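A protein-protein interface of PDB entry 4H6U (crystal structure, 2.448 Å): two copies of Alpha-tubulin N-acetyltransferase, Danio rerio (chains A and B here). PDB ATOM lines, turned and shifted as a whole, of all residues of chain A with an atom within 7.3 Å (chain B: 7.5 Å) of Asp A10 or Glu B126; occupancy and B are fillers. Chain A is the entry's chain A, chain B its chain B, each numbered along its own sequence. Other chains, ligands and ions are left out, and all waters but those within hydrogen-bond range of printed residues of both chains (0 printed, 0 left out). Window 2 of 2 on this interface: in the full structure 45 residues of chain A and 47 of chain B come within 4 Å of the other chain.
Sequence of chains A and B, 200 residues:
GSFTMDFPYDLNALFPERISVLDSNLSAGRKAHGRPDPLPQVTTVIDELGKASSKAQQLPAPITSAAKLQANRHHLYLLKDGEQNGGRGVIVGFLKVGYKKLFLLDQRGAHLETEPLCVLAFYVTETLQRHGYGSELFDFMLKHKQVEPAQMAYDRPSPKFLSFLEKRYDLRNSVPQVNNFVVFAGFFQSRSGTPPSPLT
The side-chain carboxylate (OD1) of Asp A10 sits at hydrogen-bond distance from the side-chain hydroxyl (OG1) of Thr B125 (2.6 Å). The backbone NH of Glu B126 is in hydrogen-bond range of the side-chain carboxylate of Asp A10. OD2 of Asp A10 is in hydrogen-bond range of OH of Tyr B123, at 3.0 Å. The backbone carbonyl oxygen of Phe A7 is in hydrogen-bond range of the backbone NH of Thr B43.
OE1 of Glu B126 sits close to OE1 of Gln B129 (3.5 Å). The side-chain amino group (NZ) of Lys B160 lies within salt-bridge range of the side-chain carboxylate (OE1) of Glu B126. O of Val B92 is in hydrogen-bond range of N of Thr B125. N of Phe B94 is in hydrogen-bond range of O of Tyr B123 (2.8 Å).
Among the printed residues, pairs that only touch across the chains: Phe A7 with Ile B91 (3.6 Å), Pro A8 with Pro B40 (3.9 Å), Pro A8 with Gln B41 (3.4 Å), Pro A8 with Ile B91 (2.9 Å), Pro A8 with Thr B125 (3.3 Å), Tyr A9 with Gln B41 (3.5 Å), Tyr A9 with Thr B43 (3.4 Å), Leu A11 with Ile B91 (3.7 Å), Leu A11 with Val B92 (3.6 Å), Leu A11 with Phe B94 (3.8 Å), Asn A12 with Thr B43 (3.97 Å), Leu A14 with Phe B94 (3.4 Å), Leu A14 with Tyr B123 (3.3 Å) and Phe A15 with Phe B94 (3.9 Å).
Of the printed residues of chain B, Phe A7 touches Thr B43 and Ile B91. Printed residues of chain B within 4 Å of Tyr A9: Gln B41 (3.5 Å) and Thr B43 (3.4 Å). Of chain B, only Tyr B123 (3.0 Å), Thr B125 (2.6 Å) and Glu B126 (2.8 Å) come within 4 Å of Asp A10. Printed residues of chain B within 4 Å of Phe A15: Phe B94. Of the printed residues of chain A, Gln B41 touches Pro A8 (3.4 Å) and Tyr A9 (3.5 Å). Of the printed residues of chain A, Val B92 touches Leu A11. Glu B126 touches one residue of chain A. Thr B127 touches none of the printed residues of chain A. The nearest residue of chain B that does not touch Asp A10 is Thr B127 (5.0 Å). The nearest residue of chain A that does not touch Glu B126 is Leu A11 (6.4 Å).
Of the 9 printed residues of chain A, 8 touch a printed residue of chain B. Hydrophobic or aromatic side chains of chain A that line the printed part of chain B: Phe A7, Pro A8, Tyr A9, Leu A11, Leu A14 and Phe A15. Printed residues of chain B that touch a printed residue of chain A: Pro B40, Gln B41, Thr B43, Ile B91, Val B92, Phe B94, Tyr B123, Thr B125 and Glu B126. Hydrophobic or aromatic side chains of chain B within 4 Å of the printed part of chain A: Pro B40, Ile B91, Phe B94 and Tyr B123. Along chain B the printed residues that touch a printed residue of chain A span positions 40 to 126.
No position is printed for both chains.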
ATOM      1  N   PHE A   7       9.875  16.856   1.032  1.00  0.00           N
ATOM      2  CA  PHE A   7      10.698  16.913   2.237  1.00  0.00           C
ATOM      3  C   PHE A   7      11.778  17.943   2.060  1.00  0.00           C
ATOM      4  O   PHE A   7      12.465  17.939   1.055  1.00  0.00           O
ATOM      5  CB  PHE A   7      11.409  15.562   2.502  1.00  0.00           C
ATOM      6  CG  PHE A   7      10.557  14.499   3.144  1.00  0.00           C
ATOM      7  CD1 PHE A   7       9.178  14.506   3.045  1.00  0.00           C
ATOM      8  CD2 PHE A   7      11.172  13.451   3.807  1.00  0.00           C
ATOM      9  CE1 PHE A   7       8.415  13.518   3.631  1.00  0.00           C
ATOM     10  CE2 PHE A   7      10.432  12.453   4.403  1.00  0.00           C
ATOM     11  CZ  PHE A   7       9.030  12.487   4.311  1.00  0.00           C
ATOM     12  N   PRO A   8      11.941  18.829   3.051  1.00  0.00           N
ATOM     13  CA  PRO A   8      13.150  19.664   3.066  1.00  0.00           C
ATOM     14  C   PRO A   8      14.385  18.788   3.166  1.00  0.00           C
ATOM     15  O   PRO A   8      14.283  17.731   3.768  1.00  0.00           O
ATOM     16  CB  PRO A   8      12.981  20.522   4.333  1.00  0.00           C
ATOM     17  CG  PRO A   8      11.472  20.525   4.612  1.00  0.00           C
ATOM     18  CD  PRO A   8      10.948  19.214   4.077  1.00  0.00           C
ATOM     19  N   TYR A   9      15.514  19.210   2.611  1.00  0.00           N
ATOM     20  CA  TYR A   9      16.727  18.383   2.582  1.00  0.00           C
ATOM     21  C   TYR A   9      17.256  18.002   3.955  1.00  0.00           C
ATOM     22  O   TYR A   9      17.587  16.837   4.185  1.00  0.00           O
ATOM     23  CB  TYR A   9      17.830  19.084   1.763  1.00  0.00           C
ATOM     24  CG  TYR A   9      17.581  19.062   0.264  1.00  0.00           C
ATOM     25  CD1 TYR A   9      17.329  17.854  -0.379  1.00  0.00           C
ATOM     26  CD2 TYR A   9      17.510  20.228  -0.492  1.00  0.00           C
ATOM     27  CE1 TYR A   9      17.083  17.795  -1.736  1.00  0.00           C
ATOM     28  CE2 TYR A   9      17.256  20.180  -1.858  1.00  0.00           C
ATOM     29  CZ  TYR A   9      17.032  18.952  -2.469  1.00  0.00           C
ATOM     30  OH  TYR A   9      16.777  18.839  -3.819  1.00  0.00           O
ATOM     31  N   ASP A  10      17.293  18.951   4.879  1.00  0.00           N
ATOM     32  CA  ASP A  10      17.761  18.666   6.238  1.00  0.00           C
ATOM     33  C   ASP A  10      16.822  17.658   6.910  1.00  0.00           C
ATOM     34  O   ASP A  10      17.281  16.734   7.541  1.00  0.00           O
ATOM     35  CB  ASP A  10      17.979  19.953   7.057  1.00  0.00           C
ATOM     36  CG  ASP A  10      16.698  20.741   7.296  1.00  0.00           C
ATOM     37  OD1 ASP A  10      15.673  20.460   6.634  1.00  0.00           O
ATOM     38  OD2 ASP A  10      16.732  21.665   8.128  1.00  0.00           O
ATOM     39  N   LEU A  11      15.510  17.815   6.743  1.00  0.00           N
ATOM     40  CA  LEU A  11      14.577  16.849   7.311  1.00  0.00           C
ATOM     41  C   LEU A  11      14.726  15.458   6.693  1.00  0.00           C
ATOM     42  O   LEU A  11      14.633  14.439   7.397  1.00  0.00           O
ATOM     43  CB  LEU A  11      13.166  17.347   7.134  1.00  0.00           C
ATOM     44  CG  LEU A  11      12.112  16.605   7.939  1.00  0.00           C
ATOM     45  CD1 LEU A  11      11.123  17.572   8.559  1.00  0.00           C
ATOM     46  CD2 LEU A  11      11.392  15.642   7.008  1.00  0.00           C
ATOM     47  N   ASN A  12      14.951  15.406   5.381  1.00  0.00           N
ATOM     48  CA  ASN A  12      15.092  14.138   4.698  1.00  0.00           C
ATOM     49  C   ASN A  12      16.341  13.384   5.187  1.00  0.00           C
ATOM     50  O   ASN A  12      16.311  12.180   5.435  1.00  0.00           O
ATOM     51  CB  ASN A  12      15.173  14.339   3.181  1.00  0.00           C
ATOM     52  CG  ASN A  12      14.799  13.066   2.393  1.00  0.00           C
ATOM     53  OD1 ASN A  12      13.984  12.261   2.820  1.00  0.00           O
ATOM     54  ND2 ASN A  12      15.466  12.861   1.285  1.00  0.00           N
ATOM     55  N   ALA A  13      17.443  14.112   5.298  1.00  0.00           N
ATOM     56  CA  ALA A  13      18.715  13.553   5.745  1.00  0.00           C
ATOM     57  C   ALA A  13      18.640  13.069   7.202  1.00  0.00           C
ATOM     58  O   ALA A  13      19.302  12.134   7.560  1.00  0.00           O
ATOM     59  CB  ALA A  13      19.813  14.556   5.567  1.00  0.00           C
ATOM     60  N   LEU A  14      17.881  13.747   8.053  1.00  0.00           N
ATOM     61  CA  LEU A  14      17.745  13.344   9.453  1.00  0.00           C
ATOM     62  C   LEU A  14      16.544  12.433   9.723  1.00  0.00           C
ATOM     63  O   LEU A  14      16.341  11.996  10.864  1.00  0.00           O
ATOM     64  CB  LEU A  14      17.604  14.585  10.339  1.00  0.00           C
ATOM     65  CG  LEU A  14      18.763  15.570  10.386  1.00  0.00           C
ATOM     66  CD1 LEU A  14      18.316  16.834  11.123  1.00  0.00           C
ATOM     67  CD2 LEU A  14      19.992  14.958  11.040  1.00  0.00           C
ATOM     68  N   PHE A  15      15.808  12.068   8.670  1.00  0.00           N
ATOM     69  CA  PHE A  15      14.569  11.313   8.839  1.00  0.00           C
ATOM     70  C   PHE A  15      14.844   9.999   9.580  1.00  0.00           C
ATOM     71  O   PHE A  15      15.753   9.259   9.228  1.00  0.00           O
ATOM     72  CB  PHE A  15      13.916  11.052   7.476  1.00  0.00           C
ATOM     73  CG  PHE A  15      12.444  10.696   7.561  1.00  0.00           C
ATOM     74  CD1 PHE A  15      11.495  11.657   7.868  1.00  0.00           C
ATOM     75  CD2 PHE A  15      12.020   9.388   7.297  1.00  0.00           C
ATOM     76  CE1 PHE A  15      10.142  11.337   7.952  1.00  0.00           C
ATOM     77  CE2 PHE A  15      10.679   9.044   7.353  1.00  0.00           C
ATOM     78  CZ  PHE A  15       9.722  10.030   7.685  1.00  0.00           C
ATOM     79  N   PRO B  38       9.984  31.572   5.392  1.00  0.00           N
ATOM     80  CA  PRO B  38      10.954  31.199   4.360  1.00  0.00           C
ATOM     81  C   PRO B  38      10.772  29.729   3.983  1.00  0.00           C
ATOM     82  O   PRO B  38      10.925  28.848   4.824  1.00  0.00           O
ATOM     83  CB  PRO B  38      12.303  31.432   5.047  1.00  0.00           C
ATOM     84  CG  PRO B  38      12.004  31.251   6.525  1.00  0.00           C
ATOM     85  CD  PRO B  38      10.610  31.808   6.703  1.00  0.00           C
ATOM     86  N   PRO B  40      12.113  26.356   2.721  1.00  0.00           N
ATOM     87  CA  PRO B  40      13.407  25.746   2.426  1.00  0.00           C
ATOM     88  C   PRO B  40      13.313  25.000   1.087  1.00  0.00           C
ATOM     89  O   PRO B  40      12.216  24.675   0.632  1.00  0.00           O
ATOM     90  CB  PRO B  40      13.596  24.767   3.597  1.00  0.00           C
ATOM     91  CG  PRO B  40      12.213  24.357   3.948  1.00  0.00           C
ATOM     92  CD  PRO B  40      11.349  25.595   3.726  1.00  0.00           C
ATOM     93  N   GLN B  41      14.462  24.803   0.457  1.00  0.00           N
ATOM     94  CA  GLN B  41      14.584  23.917  -0.672  1.00  0.00           C
ATOM     95  C   GLN B  41      14.070  22.514  -0.295  1.00  0.00           C
ATOM     96  O   GLN B  41      14.321  22.003   0.822  1.00  0.00           O
ATOM     97  CB  GLN B  41      16.038  23.862  -1.149  1.00  0.00           C
ATOM     98  CG  GLN B  41      16.399  24.923  -2.185  1.00  0.00           C
ATOM     99  CD  GLN B  41      17.590  24.509  -3.036  1.00  0.00           C
ATOM    100  OE1 GLN B  41      18.713  24.952  -2.805  1.00  0.00           O
ATOM    101  NE2 GLN B  41      17.349  23.642  -4.020  1.00  0.00           N
ATOM    102  N   THR B  43      12.988  18.338  -1.744  1.00  0.00           N
ATOM    103  CA  THR B  43      13.035  17.217  -2.671  1.00  0.00           C
ATOM    104  C   THR B  43      11.740  16.459  -2.568  1.00  0.00           C
ATOM    105  O   THR B  43      11.241  16.185  -1.474  1.00  0.00           O
ATOM    106  CB  THR B  43      14.177  16.219  -2.375  1.00  0.00           C
ATOM    107  OG1 THR B  43      13.886  14.956  -3.006  1.00  0.00           O
ATOM    108  CG2 THR B  43      14.315  15.976  -0.898  1.00  0.00           C
ATOM    109  N   ILE B  91       6.440  18.775   4.353  1.00  0.00           N
ATOM    110  CA  ILE B  91       6.576  18.205   5.668  1.00  0.00           C
ATOM    111  C   ILE B  91       7.626  19.021   6.414  1.00  0.00           C
ATOM    112  O   ILE B  91       8.812  19.028   6.056  1.00  0.00           O
ATOM    113  CB  ILE B  91       7.036  16.750   5.612  1.00  0.00           C
ATOM    114  CG1 ILE B  91       6.038  15.879   4.819  1.00  0.00           C
ATOM    115  CG2 ILE B  91       7.204  16.192   7.041  1.00  0.00           C
ATOM    116  CD1 ILE B  91       4.600  16.220   5.063  1.00  0.00           C
ATOM    117  N   VAL B  92       7.205  19.675   7.488  1.00  0.00           N
ATOM    118  CA  VAL B  92       8.102  20.580   8.200  1.00  0.00           C
ATOM    119  C   VAL B  92       8.683  19.998   9.482  1.00  0.00           C
ATOM    120  O   VAL B  92       9.618  20.562  10.038  1.00  0.00           O
ATOM    121  CB  VAL B  92       7.387  21.910   8.561  1.00  0.00           C
ATOM    122  CG1 VAL B  92       6.947  22.619   7.287  1.00  0.00           C
ATOM    123  CG2 VAL B  92       6.199  21.636   9.460  1.00  0.00           C
ATOM    124  N   PHE B  94       9.029  16.135  12.147  1.00  0.00           N
ATOM    125  CA  PHE B  94       8.665  14.807  12.577  1.00  0.00           C
ATOM    126  C   PHE B  94       8.968  14.596  14.056  1.00  0.00           C
ATOM    127  O   PHE B  94       9.900  15.181  14.650  1.00  0.00           O
ATOM    128  CB  PHE B  94       9.357  13.714  11.732  1.00  0.00           C
ATOM    129  CG  PHE B  94      10.877  13.729  11.828  1.00  0.00           C
ATOM    130  CD1 PHE B  94      11.529  13.287  12.970  1.00  0.00           C
ATOM    131  CD2 PHE B  94      11.644  14.205  10.786  1.00  0.00           C
ATOM    132  CE1 PHE B  94      12.915  13.304  13.056  1.00  0.00           C
ATOM    133  CE2 PHE B  94      13.015  14.220  10.865  1.00  0.00           C
ATOM    134  CZ  PHE B  94      13.656  13.778  11.997  1.00  0.00           C
ATOM    135  N   TYR B 123      12.290  16.647  15.316  1.00  0.00           N
ATOM    136  CA  TYR B 123      12.979  17.596  14.447  1.00  0.00           C
ATOM    137  C   TYR B 123      12.028  18.415  13.628  1.00  0.00           C
ATOM    138  O   TYR B 123      11.068  17.900  13.054  1.00  0.00           O
ATOM    139  CB  TYR B 123      13.980  16.903  13.499  1.00  0.00           C
ATOM    140  CG  TYR B 123      14.885  17.893  12.755  1.00  0.00           C
ATOM    141  CD1 TYR B 123      15.901  18.576  13.427  1.00  0.00           C
ATOM    142  CD2 TYR B 123      14.760  18.107  11.383  1.00  0.00           C
ATOM    143  CE1 TYR B 123      16.739  19.465  12.766  1.00  0.00           C
ATOM    144  CE2 TYR B 123      15.607  18.993  10.702  1.00  0.00           C
ATOM    145  CZ  TYR B 123      16.600  19.666  11.402  1.00  0.00           C
ATOM    146  OH  TYR B 123      17.458  20.559  10.787  1.00  0.00           O
ATOM    147  N   VAL B 124      12.321  19.704  13.578  1.00  0.00           N
ATOM    148  CA  VAL B 124      11.632  20.632  12.700  1.00  0.00           C
ATOM    149  C   VAL B 124      12.705  21.224  11.783  1.00  0.00           C
ATOM    150  O   VAL B 124      13.784  21.527  12.247  1.00  0.00           O
ATOM    151  CB  VAL B 124      10.951  21.732  13.511  1.00  0.00           C
ATOM    152  CG1 VAL B 124      10.508  22.884  12.599  1.00  0.00           C
ATOM    153  CG2 VAL B 124       9.768  21.161  14.276  1.00  0.00           C
ATOM    154  N   THR B 125      12.410  21.360  10.488  1.00  0.00           N
ATOM    155  CA  THR B 125      13.371  21.864   9.501  1.00  0.00           C
ATOM    156  C   THR B 125      13.918  23.228   9.944  1.00  0.00           C
ATOM    157  O   THR B 125      13.193  24.097  10.441  1.00  0.00           O
ATOM    158  CB  THR B 125      12.735  21.911   8.057  1.00  0.00           C
ATOM    159  OG1 THR B 125      13.764  22.119   7.079  1.00  0.00           O
ATOM    160  CG2 THR B 125      11.691  23.005   7.937  1.00  0.00           C
ATOM    161  N   GLU B 126      15.224  23.390   9.802  1.00  0.00           N
ATOM    162  CA  GLU B 126      15.955  24.451  10.486  1.00  0.00           C
ATOM    163  C   GLU B 126      15.354  25.856  10.367  1.00  0.00           C
ATOM    164  O   GLU B 126      15.159  26.540  11.371  1.00  0.00           O
ATOM    165  CB  GLU B 126      17.406  24.471   9.986  1.00  0.00           C
ATOM    166  CG  GLU B 126      18.148  25.843  10.167  1.00  0.00           C
ATOM    167  CD  GLU B 126      18.586  26.114  11.624  1.00  0.00           C
ATOM    168  OE1 GLU B 126      18.524  25.165  12.437  1.00  0.00           O
ATOM    169  OE2 GLU B 126      19.002  27.259  11.958  1.00  0.00           O
ATOM    170  N   THR B 127      15.118  26.305   9.145  1.00  0.00           N
ATOM    171  CA  THR B 127      14.644  27.671   8.908  1.00  0.00           C
ATOM    172  C   THR B 127      13.229  27.940   9.437  1.00  0.00           C
ATOM    173  O   THR B 127      12.820  29.090   9.524  1.00  0.00           O
ATOM    174  CB  THR B 127      14.661  28.015   7.403  1.00  0.00           C
ATOM    175  OG1 THR B 127      13.927  27.019   6.674  1.00  0.00           O
ATOM    176  CG2 THR B 127      16.088  28.082   6.909  1.00  0.00           C
ATOM    177  N   LEU B 128      12.509  26.894   9.831  1.00  0.00           N
ATOM    178  CA  LEU B 128      11.128  27.028  10.283  1.00  0.00           C
ATOM    179  C   LEU B 128      10.960  26.688  11.750  1.00  0.00           C
ATOM    180  O   LEU B 128       9.830  26.600  12.239  1.00  0.00           O
ATOM    181  CB  LEU B 128      10.214  26.127   9.448  1.00  0.00           C
ATOM    182  CG  LEU B 128      10.006  26.505   7.973  1.00  0.00           C
ATOM    183  CD1 LEU B 128       9.145  25.466   7.281  1.00  0.00           C
ATOM    184  CD2 LEU B 128       9.353  27.855   7.834  1.00  0.00           C
ATOM    185  N   GLN B 129      12.083  26.487  12.453  1.00  0.00           N
ATOM    186  CA  GLN B 129      12.076  26.349  13.912  1.00  0.00           C
ATOM    187  C   GLN B 129      11.579  27.656  14.562  1.00  0.00           C
ATOM    188  O   GLN B 129      11.650  28.747  13.969  1.00  0.00           O
ATOM    189  CB  GLN B 129      13.487  26.014  14.421  1.00  0.00           C
ATOM    190  CG  GLN B 129      13.805  24.519  14.430  1.00  0.00           C
ATOM    191  CD  GLN B 129      15.299  24.194  14.391  1.00  0.00           C
ATOM    192  OE1 GLN B 129      16.117  24.941  14.921  1.00  0.00           O
ATOM    193  NE2 GLN B 129      15.655  23.069  13.739  1.00  0.00           N
ATOM    194  N   ARG B 130      11.057  27.534  15.772  1.00  0.00           N
ATOM    195  CA  ARG B 130      10.583  28.685  16.523  1.00  0.00           C
ATOM    196  C   ARG B 130       9.396  29.310  15.819  1.00  0.00           C
ATOM    197  O   ARG B 130       9.223  30.530  15.877  1.00  0.00           O
ATOM    198  CB  ARG B 130      11.693  29.724  16.710  1.00  0.00           C
ATOM    199  CG  ARG B 130      12.625  29.477  17.857  1.00  0.00           C
ATOM    200  CD  ARG B 130      13.136  30.806  18.363  1.00  0.00           C
ATOM    201  NE  ARG B 130      14.569  30.814  18.616  1.00  0.00           N
ATOM    202  CZ  ARG B 130      15.117  30.868  19.829  1.00  0.00           C
ATOM    203  NH1 ARG B 130      14.352  30.908  20.916  1.00  0.00           N
ATOM    204  NH2 ARG B 130      16.435  30.880  19.950  1.00  0.00           N
ATOM    205  N   HIS B 131       8.622  28.497  15.105  1.00  0.00           N
ATOM    206  CA  HIS B 131       7.389  28.959  14.465  1.00  0.00           C
ATOM    207  C   HIS B 131       6.167  28.263  15.030  1.00  0.00           C
ATOM    208  O   HIS B 131       5.039  28.533  14.580  1.00  0.00           O
ATOM    209  CB  HIS B 131       7.428  28.695  12.941  1.00  0.00           C
ATOM    210  CG  HIS B 131       8.340  29.611  12.184  1.00  0.00           C
ATOM    211  ND1 HIS B 131       9.699  29.663  12.408  1.00  0.00           N
ATOM    212  CD2 HIS B 131       8.091  30.491  11.183  1.00  0.00           C
ATOM    213  CE1 HIS B 131      10.243  30.558  11.601  1.00  0.00           C
ATOM    214  NE2 HIS B 131       9.289  31.077  10.850  1.00  0.00           N
ATOM    215  N   LYS B 160      18.108  22.496  22.444  1.00  0.00           N
ATOM    216  CA  LYS B 160      16.886  23.112  22.005  1.00  0.00           C
ATOM    217  C   LYS B 160      15.637  22.384  22.463  1.00  0.00           C
ATOM    218  O   LYS B 160      14.603  22.998  22.766  1.00  0.00           O
ATOM    219  CB  LYS B 160      16.875  23.234  20.473  1.00  0.00           C
ATOM    220  CG  LYS B 160      17.911  24.173  19.928  1.00  0.00           C
ATOM    221  CD  LYS B 160      17.803  24.180  18.456  1.00  0.00           C
ATOM    222  CE  LYS B 160      18.942  24.917  17.794  1.00  0.00           C
ATOM    223  NZ  LYS B 160      18.826  24.753  16.307  1.00  0.00           N
